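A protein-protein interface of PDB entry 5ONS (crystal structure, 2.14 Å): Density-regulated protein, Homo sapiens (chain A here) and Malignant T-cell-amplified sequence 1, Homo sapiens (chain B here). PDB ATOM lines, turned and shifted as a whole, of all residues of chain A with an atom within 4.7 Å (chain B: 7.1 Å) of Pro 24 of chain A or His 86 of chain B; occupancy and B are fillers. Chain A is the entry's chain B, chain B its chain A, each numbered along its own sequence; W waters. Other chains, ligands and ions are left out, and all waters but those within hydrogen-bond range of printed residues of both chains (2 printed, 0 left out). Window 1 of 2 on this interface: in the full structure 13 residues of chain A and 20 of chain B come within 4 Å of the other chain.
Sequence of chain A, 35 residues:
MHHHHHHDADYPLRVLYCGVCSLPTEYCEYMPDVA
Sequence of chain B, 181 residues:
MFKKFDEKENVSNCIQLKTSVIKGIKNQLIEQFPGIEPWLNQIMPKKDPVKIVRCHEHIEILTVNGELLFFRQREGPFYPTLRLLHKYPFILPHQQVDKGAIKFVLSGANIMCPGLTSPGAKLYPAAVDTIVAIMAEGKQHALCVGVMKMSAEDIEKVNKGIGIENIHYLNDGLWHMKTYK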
ATOM      1  N   LEU A  13      -3.880 -31.871  20.006  1.00  0.00           N
ATOM      2  CA  LEU A  13      -2.899 -32.938  20.160  1.00  0.00           C
ATOM      3  C   LEU A  13      -2.735 -33.271  21.644  1.00  0.00           C
ATOM      4  O   LEU A  13      -2.851 -32.406  22.518  1.00  0.00           O
ATOM      5  CB  LEU A  13      -1.555 -32.526  19.544  1.00  0.00           C
ATOM      6  CG  LEU A  13      -1.656 -31.939  18.120  1.00  0.00           C
ATOM      7  CD1 LEU A  13      -0.288 -31.632  17.553  1.00  0.00           C
ATOM      8  CD2 LEU A  13      -2.406 -32.899  17.196  1.00  0.00           C
ATOM      9  N   VAL A  15       0.113 -34.631  23.814  1.00  0.00           N
ATOM     10  CA  VAL A  15       1.546 -34.878  23.818  1.00  0.00           C
ATOM     11  C   VAL A  15       1.888 -35.595  25.118  1.00  0.00           C
ATOM     12  O   VAL A  15       1.453 -35.171  26.195  1.00  0.00           O
ATOM     13  CB  VAL A  15       2.321 -33.557  23.678  1.00  0.00           C
ATOM     14  CG1 VAL A  15       3.810 -33.791  23.681  1.00  0.00           C
ATOM     15  CG2 VAL A  15       1.893 -32.833  22.396  1.00  0.00           C
ATOM     16  N   LEU A  16       2.637 -36.696  25.018  1.00  0.00           N
ATOM     17  CA  LEU A  16       3.049 -37.445  26.202  1.00  0.00           C
ATOM     18  C   LEU A  16       4.198 -36.721  26.892  1.00  0.00           C
ATOM     19  O   LEU A  16       5.228 -36.433  26.273  1.00  0.00           O
ATOM     20  CB  LEU A  16       3.472 -38.873  25.836  1.00  0.00           C
ATOM     21  CG  LEU A  16       4.264 -39.680  26.898  1.00  0.00           C
ATOM     22  CD1 LEU A  16       3.409 -40.109  28.102  1.00  0.00           C
ATOM     23  CD2 LEU A  16       4.971 -40.901  26.294  1.00  0.00           C
ATOM     24  N   TYR A  17       4.023 -36.429  28.174  1.00  0.00           N
ATOM     25  CA  TYR A  17       5.046 -35.757  28.961  1.00  0.00           C
ATOM     26  C   TYR A  17       5.670 -36.752  29.928  1.00  0.00           C
ATOM     27  O   TYR A  17       4.964 -37.440  30.679  1.00  0.00           O
ATOM     28  CB  TYR A  17       4.473 -34.549  29.704  1.00  0.00           C
ATOM     29  CG  TYR A  17       3.992 -33.443  28.763  1.00  0.00           C
ATOM     30  CD1 TYR A  17       4.881 -32.798  27.911  1.00  0.00           C
ATOM     31  CD2 TYR A  17       2.660 -33.055  28.734  1.00  0.00           C
ATOM     32  CE1 TYR A  17       4.465 -31.802  27.061  1.00  0.00           C
ATOM     33  CE2 TYR A  17       2.230 -32.046  27.888  1.00  0.00           C
ATOM     34  CZ  TYR A  17       3.135 -31.423  27.061  1.00  0.00           C
ATOM     35  OH  TYR A  17       2.696 -30.428  26.223  1.00  0.00           O
ATOM     36  N   SER A  22       9.165 -34.248  33.175  1.00  0.00           N
ATOM     37  CA  SER A  22       7.947 -33.536  32.764  1.00  0.00           C
ATOM     38  C   SER A  22       7.993 -32.975  31.340  1.00  0.00           C
ATOM     39  O   SER A  22       7.051 -32.280  30.930  1.00  0.00           O
ATOM     40  CB  SER A  22       7.580 -32.381  33.706  1.00  0.00           C
ATOM     41  OG  SER A  22       8.172 -31.167  33.257  1.00  0.00           O
ATOM     42  N   LEU A  23       9.028 -33.250  30.583  1.00  0.00           N
ATOM     43  CA  LEU A  23       9.243 -32.780  29.224  1.00  0.00           C
ATOM     44  C   LEU A  23       8.697 -33.774  28.212  1.00  0.00           C
ATOM     45  O   LEU A  23       8.448 -34.935  28.552  1.00  0.00           O
ATOM     46  CB  LEU A  23      10.732 -32.562  28.994  1.00  0.00           C
ATOM     47  CG  LEU A  23      11.252 -31.189  29.407  1.00  0.00           C
ATOM     48  CD1 LEU A  23      10.728 -30.758  30.762  1.00  0.00           C
ATOM     49  CD2 LEU A  23      12.750 -31.243  29.448  1.00  0.00           C
ATOM     50  N   PRO A  24       8.463 -33.350  26.963  1.00  0.00           N
ATOM     51  CA  PRO A  24       8.245 -34.337  25.895  1.00  0.00           C
ATOM     52  C   PRO A  24       9.438 -35.278  25.840  1.00  0.00           C
ATOM     53  O   PRO A  24      10.583 -34.848  25.986  1.00  0.00           O
ATOM     54  CB  PRO A  24       8.134 -33.481  24.628  1.00  0.00           C
ATOM     55  CG  PRO A  24       7.710 -32.131  25.128  1.00  0.00           C
ATOM     56  CD  PRO A  24       8.408 -31.968  26.449  1.00  0.00           C
ATOM     57  N   THR A  25       9.161 -36.577  25.649  1.00  0.00           N
ATOM     58  CA  THR A  25      10.199 -37.595  25.828  1.00  0.00           C
ATOM     59  C   THR A  25      11.362 -37.433  24.856  1.00  0.00           C
ATOM     60  O   THR A  25      12.406 -38.070  25.053  1.00  0.00           O
ATOM     61  CB  THR A  25       9.617 -39.017  25.695  1.00  0.00           C
ATOM     62  OG1 THR A  25       8.958 -39.170  24.428  1.00  0.00           O
ATOM     63  CG2 THR A  25       8.641 -39.318  26.834  1.00  0.00           C
ATOM     64  N   GLU A  26      11.209 -36.602  23.822  1.00  0.00           N
ATOM     65  CA  GLU A  26      12.304 -36.275  22.920  1.00  0.00           C
ATOM     66  C   GLU A  26      13.269 -35.252  23.509  1.00  0.00           C
ATOM     67  O   GLU A  26      14.337 -35.030  22.924  1.00  0.00           O
ATOM     68  CB  GLU A  26      11.745 -35.749  21.596  1.00  0.00           C
ATOM     69  CG  GLU A  26      11.121 -34.376  21.717  1.00  0.00           C
ATOM     70  CD  GLU A  26      10.335 -33.971  20.480  1.00  0.00           C
ATOM     71  OE1 GLU A  26       9.502 -33.046  20.588  1.00  0.00           O
ATOM     72  OE2 GLU A  26      10.543 -34.572  19.402  1.00  0.00           O
ATOM     73  N   TYR A  27      12.909 -34.613  24.628  1.00  0.00           N
ATOM     74  CA  TYR A  27      13.788 -33.695  25.347  1.00  0.00           C
ATOM     75  C   TYR A  27      14.382 -34.281  26.623  1.00  0.00           C
ATOM     76  O   TYR A  27      15.193 -33.606  27.270  1.00  0.00           O
ATOM     77  CB  TYR A  27      13.040 -32.401  25.694  1.00  0.00           C
ATOM     78  CG  TYR A  27      12.760 -31.597  24.456  1.00  0.00           C
ATOM     79  CD1 TYR A  27      13.781 -30.887  23.841  1.00  0.00           C
ATOM     80  CD2 TYR A  27      11.493 -31.581  23.874  1.00  0.00           C
ATOM     81  CE1 TYR A  27      13.560 -30.160  22.697  1.00  0.00           C
ATOM     82  CE2 TYR A  27      11.250 -30.837  22.706  1.00  0.00           C
ATOM     83  CZ  TYR A  27      12.299 -30.134  22.125  1.00  0.00           C
ATOM     84  OH  TYR A  27      12.126 -29.397  20.975  1.00  0.00           O
ATOM     85  N   CYS A  28      13.990 -35.500  27.007  1.00  0.00           N
ATOM     86  CA  CYS A  28      14.604 -36.187  28.144  1.00  0.00           C
ATOM     87  C   CYS A  28      16.123 -36.095  28.092  1.00  0.00           C
ATOM     88  O   CYS A  28      16.781 -35.844  29.109  1.00  0.00           O
ATOM     89  CB  CYS A  28      14.183 -37.657  28.154  1.00  0.00           C
ATOM     90  SG  CYS A  28      12.502 -37.987  28.661  1.00  0.00           S
ATOM     91  N   THR B  81       0.943 -20.328  26.222  1.00  0.00           N
ATOM     92  CA  THR B  81       1.867 -21.202  26.944  1.00  0.00           C
ATOM     93  C   THR B  81       2.356 -22.300  26.012  1.00  0.00           C
ATOM     94  O   THR B  81       1.715 -22.626  25.009  1.00  0.00           O
ATOM     95  CB  THR B  81       1.207 -21.843  28.169  1.00  0.00           C
ATOM     96  OG1 THR B  81       0.078 -22.663  27.753  1.00  0.00           O
ATOM     97  CG2 THR B  81       0.747 -20.759  29.153  1.00  0.00           C
ATOM     98  N   LEU B  82       3.491 -22.905  26.376  1.00  0.00           N
ATOM     99  CA  LEU B  82       3.993 -24.029  25.596  1.00  0.00           C
ATOM    100  C   LEU B  82       3.048 -25.219  25.661  1.00  0.00           C
ATOM    101  O   LEU B  82       2.944 -25.973  24.688  1.00  0.00           O
ATOM    102  CB  LEU B  82       5.403 -24.417  26.070  1.00  0.00           C
ATOM    103  CG  LEU B  82       6.530 -23.524  25.522  1.00  0.00           C
ATOM    104  CD1 LEU B  82       7.830 -23.687  26.309  1.00  0.00           C
ATOM    105  CD2 LEU B  82       6.772 -23.726  23.996  1.00  0.00           C
ATOM    106  N   ARG B  83       2.346 -25.407  26.789  1.00  0.00           N
ATOM    107  CA  ARG B  83       1.388 -26.510  26.884  1.00  0.00           C
ATOM    108  C   ARG B  83       0.221 -26.317  25.914  1.00  0.00           C
ATOM    109  O   ARG B  83      -0.265 -27.280  25.312  1.00  0.00           O
ATOM    110  CB  ARG B  83       0.871 -26.626  28.316  1.00  0.00           C
ATOM    111  CG  ARG B  83       1.913 -27.272  29.303  1.00  0.00           C
ATOM    112  CD  ARG B  83       1.398 -27.426  30.738  1.00  0.00           C
ATOM    113  NE  ARG B  83       2.535 -27.670  31.636  1.00  0.00           N
ATOM    114  CZ  ARG B  83       3.152 -28.846  31.734  1.00  0.00           C
ATOM    115  NH1 ARG B  83       2.716 -29.883  31.008  1.00  0.00           N
ATOM    116  NH2 ARG B  83       4.204 -28.986  32.539  1.00  0.00           N
ATOM    117  N   LEU B  84      -0.284 -25.091  25.799  1.00  0.00           N
ATOM    118  CA  LEU B  84      -1.346 -24.831  24.836  1.00  0.00           C
ATOM    119  C   LEU B  84      -0.820 -24.993  23.417  1.00  0.00           C
ATOM    120  O   LEU B  84      -1.462 -25.635  22.576  1.00  0.00           O
ATOM    121  CB  LEU B  84      -1.925 -23.429  25.045  1.00  0.00           C
ATOM    122  CG  LEU B  84      -3.076 -23.079  24.079  1.00  0.00           C
ATOM    123  CD1 LEU B  84      -4.255 -24.038  24.254  1.00  0.00           C
ATOM    124  CD2 LEU B  84      -3.527 -21.664  24.307  1.00  0.00           C
ATOM    125  N   LEU B  85       0.380 -24.453  23.157  1.00  0.00           N
ATOM    126  CA  LEU B  85       1.003 -24.571  21.841  1.00  0.00           C
ATOM    127  C   LEU B  85       1.212 -26.031  21.453  1.00  0.00           C
ATOM    128  O   LEU B  85       1.002 -26.401  20.293  1.00  0.00           O
ATOM    129  CB  LEU B  85       2.328 -23.803  21.833  1.00  0.00           C
ATOM    130  CG  LEU B  85       3.077 -23.522  20.526  1.00  0.00           C
ATOM    131  CD1 LEU B  85       2.188 -22.835  19.414  1.00  0.00           C
ATOM    132  CD2 LEU B  85       4.274 -22.662  20.866  1.00  0.00           C
ATOM    133  N   HIS B  86       1.590 -26.891  22.411  1.00  0.00           N
ATOM    134  CA  HIS B  86       1.756 -28.297  22.063  1.00  0.00           C
ATOM    135  C   HIS B  86       0.439 -28.918  21.617  1.00  0.00           C
ATOM    136  O   HIS B  86       0.427 -29.869  20.818  1.00  0.00           O
ATOM    137  CB  HIS B  86       2.339 -29.074  23.255  1.00  0.00           C
ATOM    138  CG  HIS B  86       3.806 -28.844  23.438  1.00  0.00           C
ATOM    139  ND1 HIS B  86       4.521 -29.349  24.503  1.00  0.00           N
ATOM    140  CD2 HIS B  86       4.689 -28.148  22.682  1.00  0.00           C
ATOM    141  CE1 HIS B  86       5.785 -28.974  24.393  1.00  0.00           C
ATOM    142  NE2 HIS B  86       5.911 -28.239  23.299  1.00  0.00           N
ATOM    143  N   LYS B  87      -0.671 -28.431  22.156  1.00  0.00           N
ATOM    144  CA  LYS B  87      -1.972 -28.940  21.753  1.00  0.00           C
ATOM    145  C   LYS B  87      -2.412 -28.353  20.422  1.00  0.00           C
ATOM    146  O   LYS B  87      -3.179 -28.992  19.685  1.00  0.00           O
ATOM    147  CB  LYS B  87      -3.021 -28.600  22.810  1.00  0.00           C
ATOM    148  CG  LYS B  87      -2.818 -29.241  24.152  1.00  0.00           C
ATOM    149  CD  LYS B  87      -3.797 -28.625  25.127  1.00  0.00           C
ATOM    150  CE  LYS B  87      -3.964 -29.478  26.352  1.00  0.00           C
ATOM    151  NZ  LYS B  87      -5.098 -28.956  27.150  1.00  0.00           N
ATOM    152  N   TYR B  88      -1.952 -27.140  20.113  1.00  0.00           N
ATOM    153  CA  TYR B  88      -2.375 -26.412  18.905  1.00  0.00           C
ATOM    154  C   TYR B  88      -1.152 -25.753  18.277  1.00  0.00           C
ATOM    155  O   TYR B  88      -0.944 -24.544  18.409  1.00  0.00           O
ATOM    156  CB  TYR B  88      -3.434 -25.362  19.247  1.00  0.00           C
ATOM    157  CG  TYR B  88      -4.696 -25.905  19.867  1.00  0.00           C
ATOM    158  CD1 TYR B  88      -5.761 -26.360  19.064  1.00  0.00           C
ATOM    159  CD2 TYR B  88      -4.850 -25.933  21.254  1.00  0.00           C
ATOM    160  CE1 TYR B  88      -6.919 -26.850  19.640  1.00  0.00           C
ATOM    161  CE2 TYR B  88      -6.006 -26.437  21.845  1.00  0.00           C
ATOM    162  CZ  TYR B  88      -7.026 -26.891  21.043  1.00  0.00           C
ATOM    163  OH  TYR B  88      -8.166 -27.368  21.633  1.00  0.00           O
ATOM    164  N   PRO B  89      -0.277 -26.540  17.639  1.00  0.00           N
ATOM    165  CA  PRO B  89       1.028 -25.993  17.218  1.00  0.00           C
ATOM    166  C   PRO B  89       0.927 -24.906  16.172  1.00  0.00           C
ATOM    167  O   PRO B  89       1.883 -24.134  16.005  1.00  0.00           O
ATOM    168  CB  PRO B  89       1.774 -27.216  16.664  1.00  0.00           C
ATOM    169  CG  PRO B  89       1.060 -28.416  17.202  1.00  0.00           C
ATOM    170  CD  PRO B  89      -0.382 -27.994  17.401  1.00  0.00           C
ATOM    171  N   ILE B  91      -0.932 -22.247  16.068  1.00  0.00           N
ATOM    172  CA  ILE B  91      -1.280 -20.935  16.603  1.00  0.00           C
ATOM    173  C   ILE B  91      -0.260 -19.886  16.216  1.00  0.00           C
ATOM    174  O   ILE B  91      -0.589 -18.702  16.160  1.00  0.00           O
ATOM    175  CB  ILE B  91      -1.367 -21.013  18.150  1.00  0.00           C
ATOM    176  CG1 ILE B  91      -2.630 -21.689  18.635  1.00  0.00           C
ATOM    177  CG2 ILE B  91      -1.289 -19.635  18.804  1.00  0.00           C
ATOM    178  CD1 ILE B  91      -2.626 -21.762  20.199  1.00  0.00           C
ATOM    179  N   GLN B 140      10.132 -32.816  17.276  1.00  0.00           N
ATOM    180  CA  GLN B 140       8.758 -32.656  16.823  1.00  0.00           C
ATOM    181  C   GLN B 140       8.025 -31.536  17.551  1.00  0.00           C
ATOM    182  O   GLN B 140       7.136 -30.904  16.965  1.00  0.00           O
ATOM    183  CB  GLN B 140       8.014 -33.981  17.009  1.00  0.00           C
ATOM    184  CG  GLN B 140       6.494 -33.891  16.941  1.00  0.00           C
ATOM    185  CD  GLN B 140       5.826 -35.254  17.001  1.00  0.00           C
ATOM    186  OE1 GLN B 140       6.494 -36.288  16.931  1.00  0.00           O
ATOM    187  NE2 GLN B 140       4.502 -35.262  17.128  1.00  0.00           N
ATOM    188  N   HIS B 141       8.363 -31.263  18.811  1.00  0.00           N
ATOM    189  CA  HIS B 141       7.588 -30.319  19.602  1.00  0.00           C
ATOM    190  C   HIS B 141       8.359 -29.024  19.842  1.00  0.00           C
ATOM    191  O   HIS B 141       9.592 -29.008  19.881  1.00  0.00           O
ATOM    192  CB  HIS B 141       7.165 -30.948  20.930  1.00  0.00           C
ATOM    193  CG  HIS B 141       6.364 -32.202  20.763  1.00  0.00           C
ATOM    194  ND1 HIS B 141       6.916 -33.461  20.895  1.00  0.00           N
ATOM    195  CD2 HIS B 141       5.058 -32.392  20.460  1.00  0.00           C
ATOM    196  CE1 HIS B 141       5.982 -34.371  20.685  1.00  0.00           C
ATOM    197  NE2 HIS B 141       4.845 -33.751  20.421  1.00  0.00           N
ATOM    198  N   ALA B 142       7.611 -27.929  19.980  1.00  0.00           N
ATOM    199  CA  ALA B 142       8.216 -26.638  20.301  1.00  0.00           C
ATOM    200  C   ALA B 142       8.836 -26.658  21.703  1.00  0.00           C
ATOM    201  O   ALA B 142       8.336 -27.309  22.627  1.00  0.00           O
ATOM    202  CB  ALA B 142       7.166 -25.518  20.205  1.00  0.00           C
ATOM    203  N   LEU B 143       9.927 -25.910  21.861  1.00  0.00           N
ATOM    204  CA  LEU B 143      10.647 -25.828  23.124  1.00  0.00           C
ATOM    205  C   LEU B 143      10.722 -24.412  23.686  1.00  0.00           C
ATOM    206  O   LEU B 143      11.264 -24.221  24.779  1.00  0.00           O
ATOM    207  CB  LEU B 143      12.065 -26.403  22.964  1.00  0.00           C
ATOM    208  CG  LEU B 143      13.200 -25.507  22.452  1.00  0.00           C
ATOM    209  CD1 LEU B 143      14.505 -26.257  22.517  1.00  0.00           C
ATOM    210  CD2 LEU B 143      12.954 -25.058  21.035  1.00  0.00           C
ATOM    211  N   CYS B 144      10.187 -23.416  22.986  1.00  0.00           N
ATOM    212  CA  CYS B 144      10.343 -22.036  23.413  1.00  0.00           C
ATOM    213  C   CYS B 144       9.327 -21.166  22.683  1.00  0.00           C
ATOM    214  O   CYS B 144       9.015 -21.409  21.513  1.00  0.00           O
ATOM    215  CB  CYS B 144      11.781 -21.557  23.150  1.00  0.00           C
ATOM    216  SG  CYS B 144      12.093 -19.819  23.430  1.00  0.00           S
ATOM    217  N   LEU B 170      10.715 -24.727  27.738  1.00  0.00           N
ATOM    218  CA  LEU B 170      10.421 -25.970  28.441  1.00  0.00           C
ATOM    219  C   LEU B 170      11.194 -26.022  29.751  1.00  0.00           C
ATOM    220  O   LEU B 170      12.363 -25.626  29.815  1.00  0.00           O
ATOM    221  CB  LEU B 170      10.777 -27.185  27.586  1.00  0.00           C
ATOM    222  CG  LEU B 170      10.019 -27.450  26.293  1.00  0.00           C
ATOM    223  CD1 LEU B 170      10.619 -28.684  25.630  1.00  0.00           C
ATOM    224  CD2 LEU B 170       8.536 -27.617  26.537  1.00  0.00           C
ATOM    225  N   TRP B 175       6.515 -23.468  32.990  1.00  0.00           N
ATOM    226  CA  TRP B 175       6.290 -24.855  32.618  1.00  0.00           C
ATOM    227  C   TRP B 175       6.062 -25.730  33.852  1.00  0.00           C
ATOM    228  O   TRP B 175       5.167 -26.586  33.850  1.00  0.00           O
ATOM    229  CB  TRP B 175       7.466 -25.353  31.784  1.00  0.00           C
ATOM    230  CG  TRP B 175       7.299 -26.790  31.364  1.00  0.00           C
ATOM    231  CD1 TRP B 175       7.801 -27.903  32.008  1.00  0.00           C
ATOM    232  CD2 TRP B 175       6.573 -27.276  30.225  1.00  0.00           C
ATOM    233  NE1 TRP B 175       7.435 -29.037  31.328  1.00  0.00           N
ATOM    234  CE2 TRP B 175       6.679 -28.687  30.235  1.00  0.00           C
ATOM    235  CE3 TRP B 175       5.832 -26.661  29.206  1.00  0.00           C
ATOM    236  CZ2 TRP B 175       6.083 -29.492  29.254  1.00  0.00           C
ATOM    237  CZ3 TRP B 175       5.243 -27.469  28.220  1.00  0.00           C
ATOM    238  CH2 TRP B 175       5.375 -28.862  28.256  1.00  0.00           C
HETATM  239  O   HOH W   1       4.543 -31.754  32.019  1.00  0.00           O
HETATM  240  O   HOH W   2       0.087 -29.874  26.137  1.00  0.00           O
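Of the 17 printed residues of chain B, 9 touch a printed residue of chain A. Hydrophobic or aromatic side chains of chain B within 4 Å of the printed part of chain A: His 86, Pro 89, His 141, Leu 143, Leu 170 and Trp 175. Of the 11 printed residues of chain A, 8 touch a printed residue of chain B. Printed residues of chain A that touch a printed residue of chain B: Leu 13, Val 15, Tyr 17, Ser 22, Leu 23, Pro 24, Glu 26 and Tyr 27.
Water W2 bridges the side-chain hydroxyl of Tyr 17 of chain A (2.7 Å) and the backbone carbonyl oxygen of Arg 83 of chain B (2.7 Å). Water W1 lies within hydrogen-bond range of O of Ser 22 of chain A (2.8 Å) and NH1 of Arg 83 of chain B (2.8 Å).
The backbone carbonyl oxygen (O) of His 141 of chain B is in hydrogen-bond range of the side-chain hydroxyl (OH) of Tyr 27 of chain A, at 2.8 Å. A ring nitrogen (ND1) of His 141 of chain B lies within hydrogen-bond range of the side-chain carboxylate (OE1) of Glu 26 of chain A. The indole nitrogen of Trp 175 of chain B sits at hydrogen-bond distance from the side-chain hydroxyl of Ser 22 of chain A, 3.0 Å away. The backbone carbonyl oxygen (O) of Lys 87 of chain B is in hydrogen-bond range of the backbone NH (N) of Leu 13 of chain A. The side-chain carboxylate (OE2) of Glu 26 of chain A is in hydrogen-bond range of the backbone NH (N) of Gln 140 of chain B (2.8 Å). The side-chain hydroxyl of Tyr 17 of chain A sits at hydrogen-bond distance from a ring nitrogen (ND1) of His 86 of chain B.
The backbone carbonyl oxygen (O) of Ala 142 of chain B sits at hydrogen-bond distance from a ring nitrogen (NE2) of His 86 of chain B (2.7 Å). The guanidinium group (NH2) of Arg 83 of chain B sits at hydrogen-bond distance from the backbone carbonyl oxygen (O) of Trp 175 of chain B (2.9 Å). The backbone carbonyl oxygen (O) of Leu 143 of chain B is in hydrogen-bond range of the backbone NH (N) of Leu 170 of chain B (3.1 Å).
Printed residues of chain B within 4 Å of Tyr 17 of chain A: Arg 83 (3.8 Å), His 86 (2.7 Å) and Trp 175 (3.3 Å). Of the printed residues of chain B, Ser 22 of chain A touches Trp 175. Pro 24 of chain A touches just these residues of chain B: His 86 (3.8 Å) and His 141 (3.9 Å). Leu 82 of chain B touches none of the printed residues of chain A. Of the printed residues of chain A, Arg 83 of chain B touches Tyr 17 (3.8 Å). Leu 84 of chain B touches none of the printed residues of chain A. Printed residues of chain A within 4 Å of Pro 89 of chain B: Leu 13 (3.5 Å). Of the printed residues of chain A, Trp 175 of chain B touches Tyr 17 (3.3 Å), Ser 22 (3.0 Å) and Leu 23 (3.8 Å). The nearest printed residue of chain A that does not touch His 86 of chain B is Tyr 27 of chain A (6.0 Å).
Among the printed residues, pairs that only touch across the chains: Tyr 17 of chain A with Trp 175 of chain B (3.3 Å), Val 15 of chain A with His 141 of chain B (3.4 Å), Tyr 27 of chain A with Leu 170 of chain B (3.5 Å), Leu 13 of chain A with Pro 89 of chain B (3.5 Å), Leu 13 of chain A with His 86 of chain B (3.6 Å), Tyr 27 of chain A with Leu 143 of chain B (3.6 Å), Val 15 of chain A with His 86 of chain B (3.7 Å), Leu 23 of chain A with Trp 175 of chain B (3.8 Å), Pro 24 of chain A with His 86 of chain B (3.8 Å), Tyr 17 of chain A with Arg 83 of chain B (3.8 Å) and Pro 24 of chain A with His 141 of chain B (3.9 Å).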
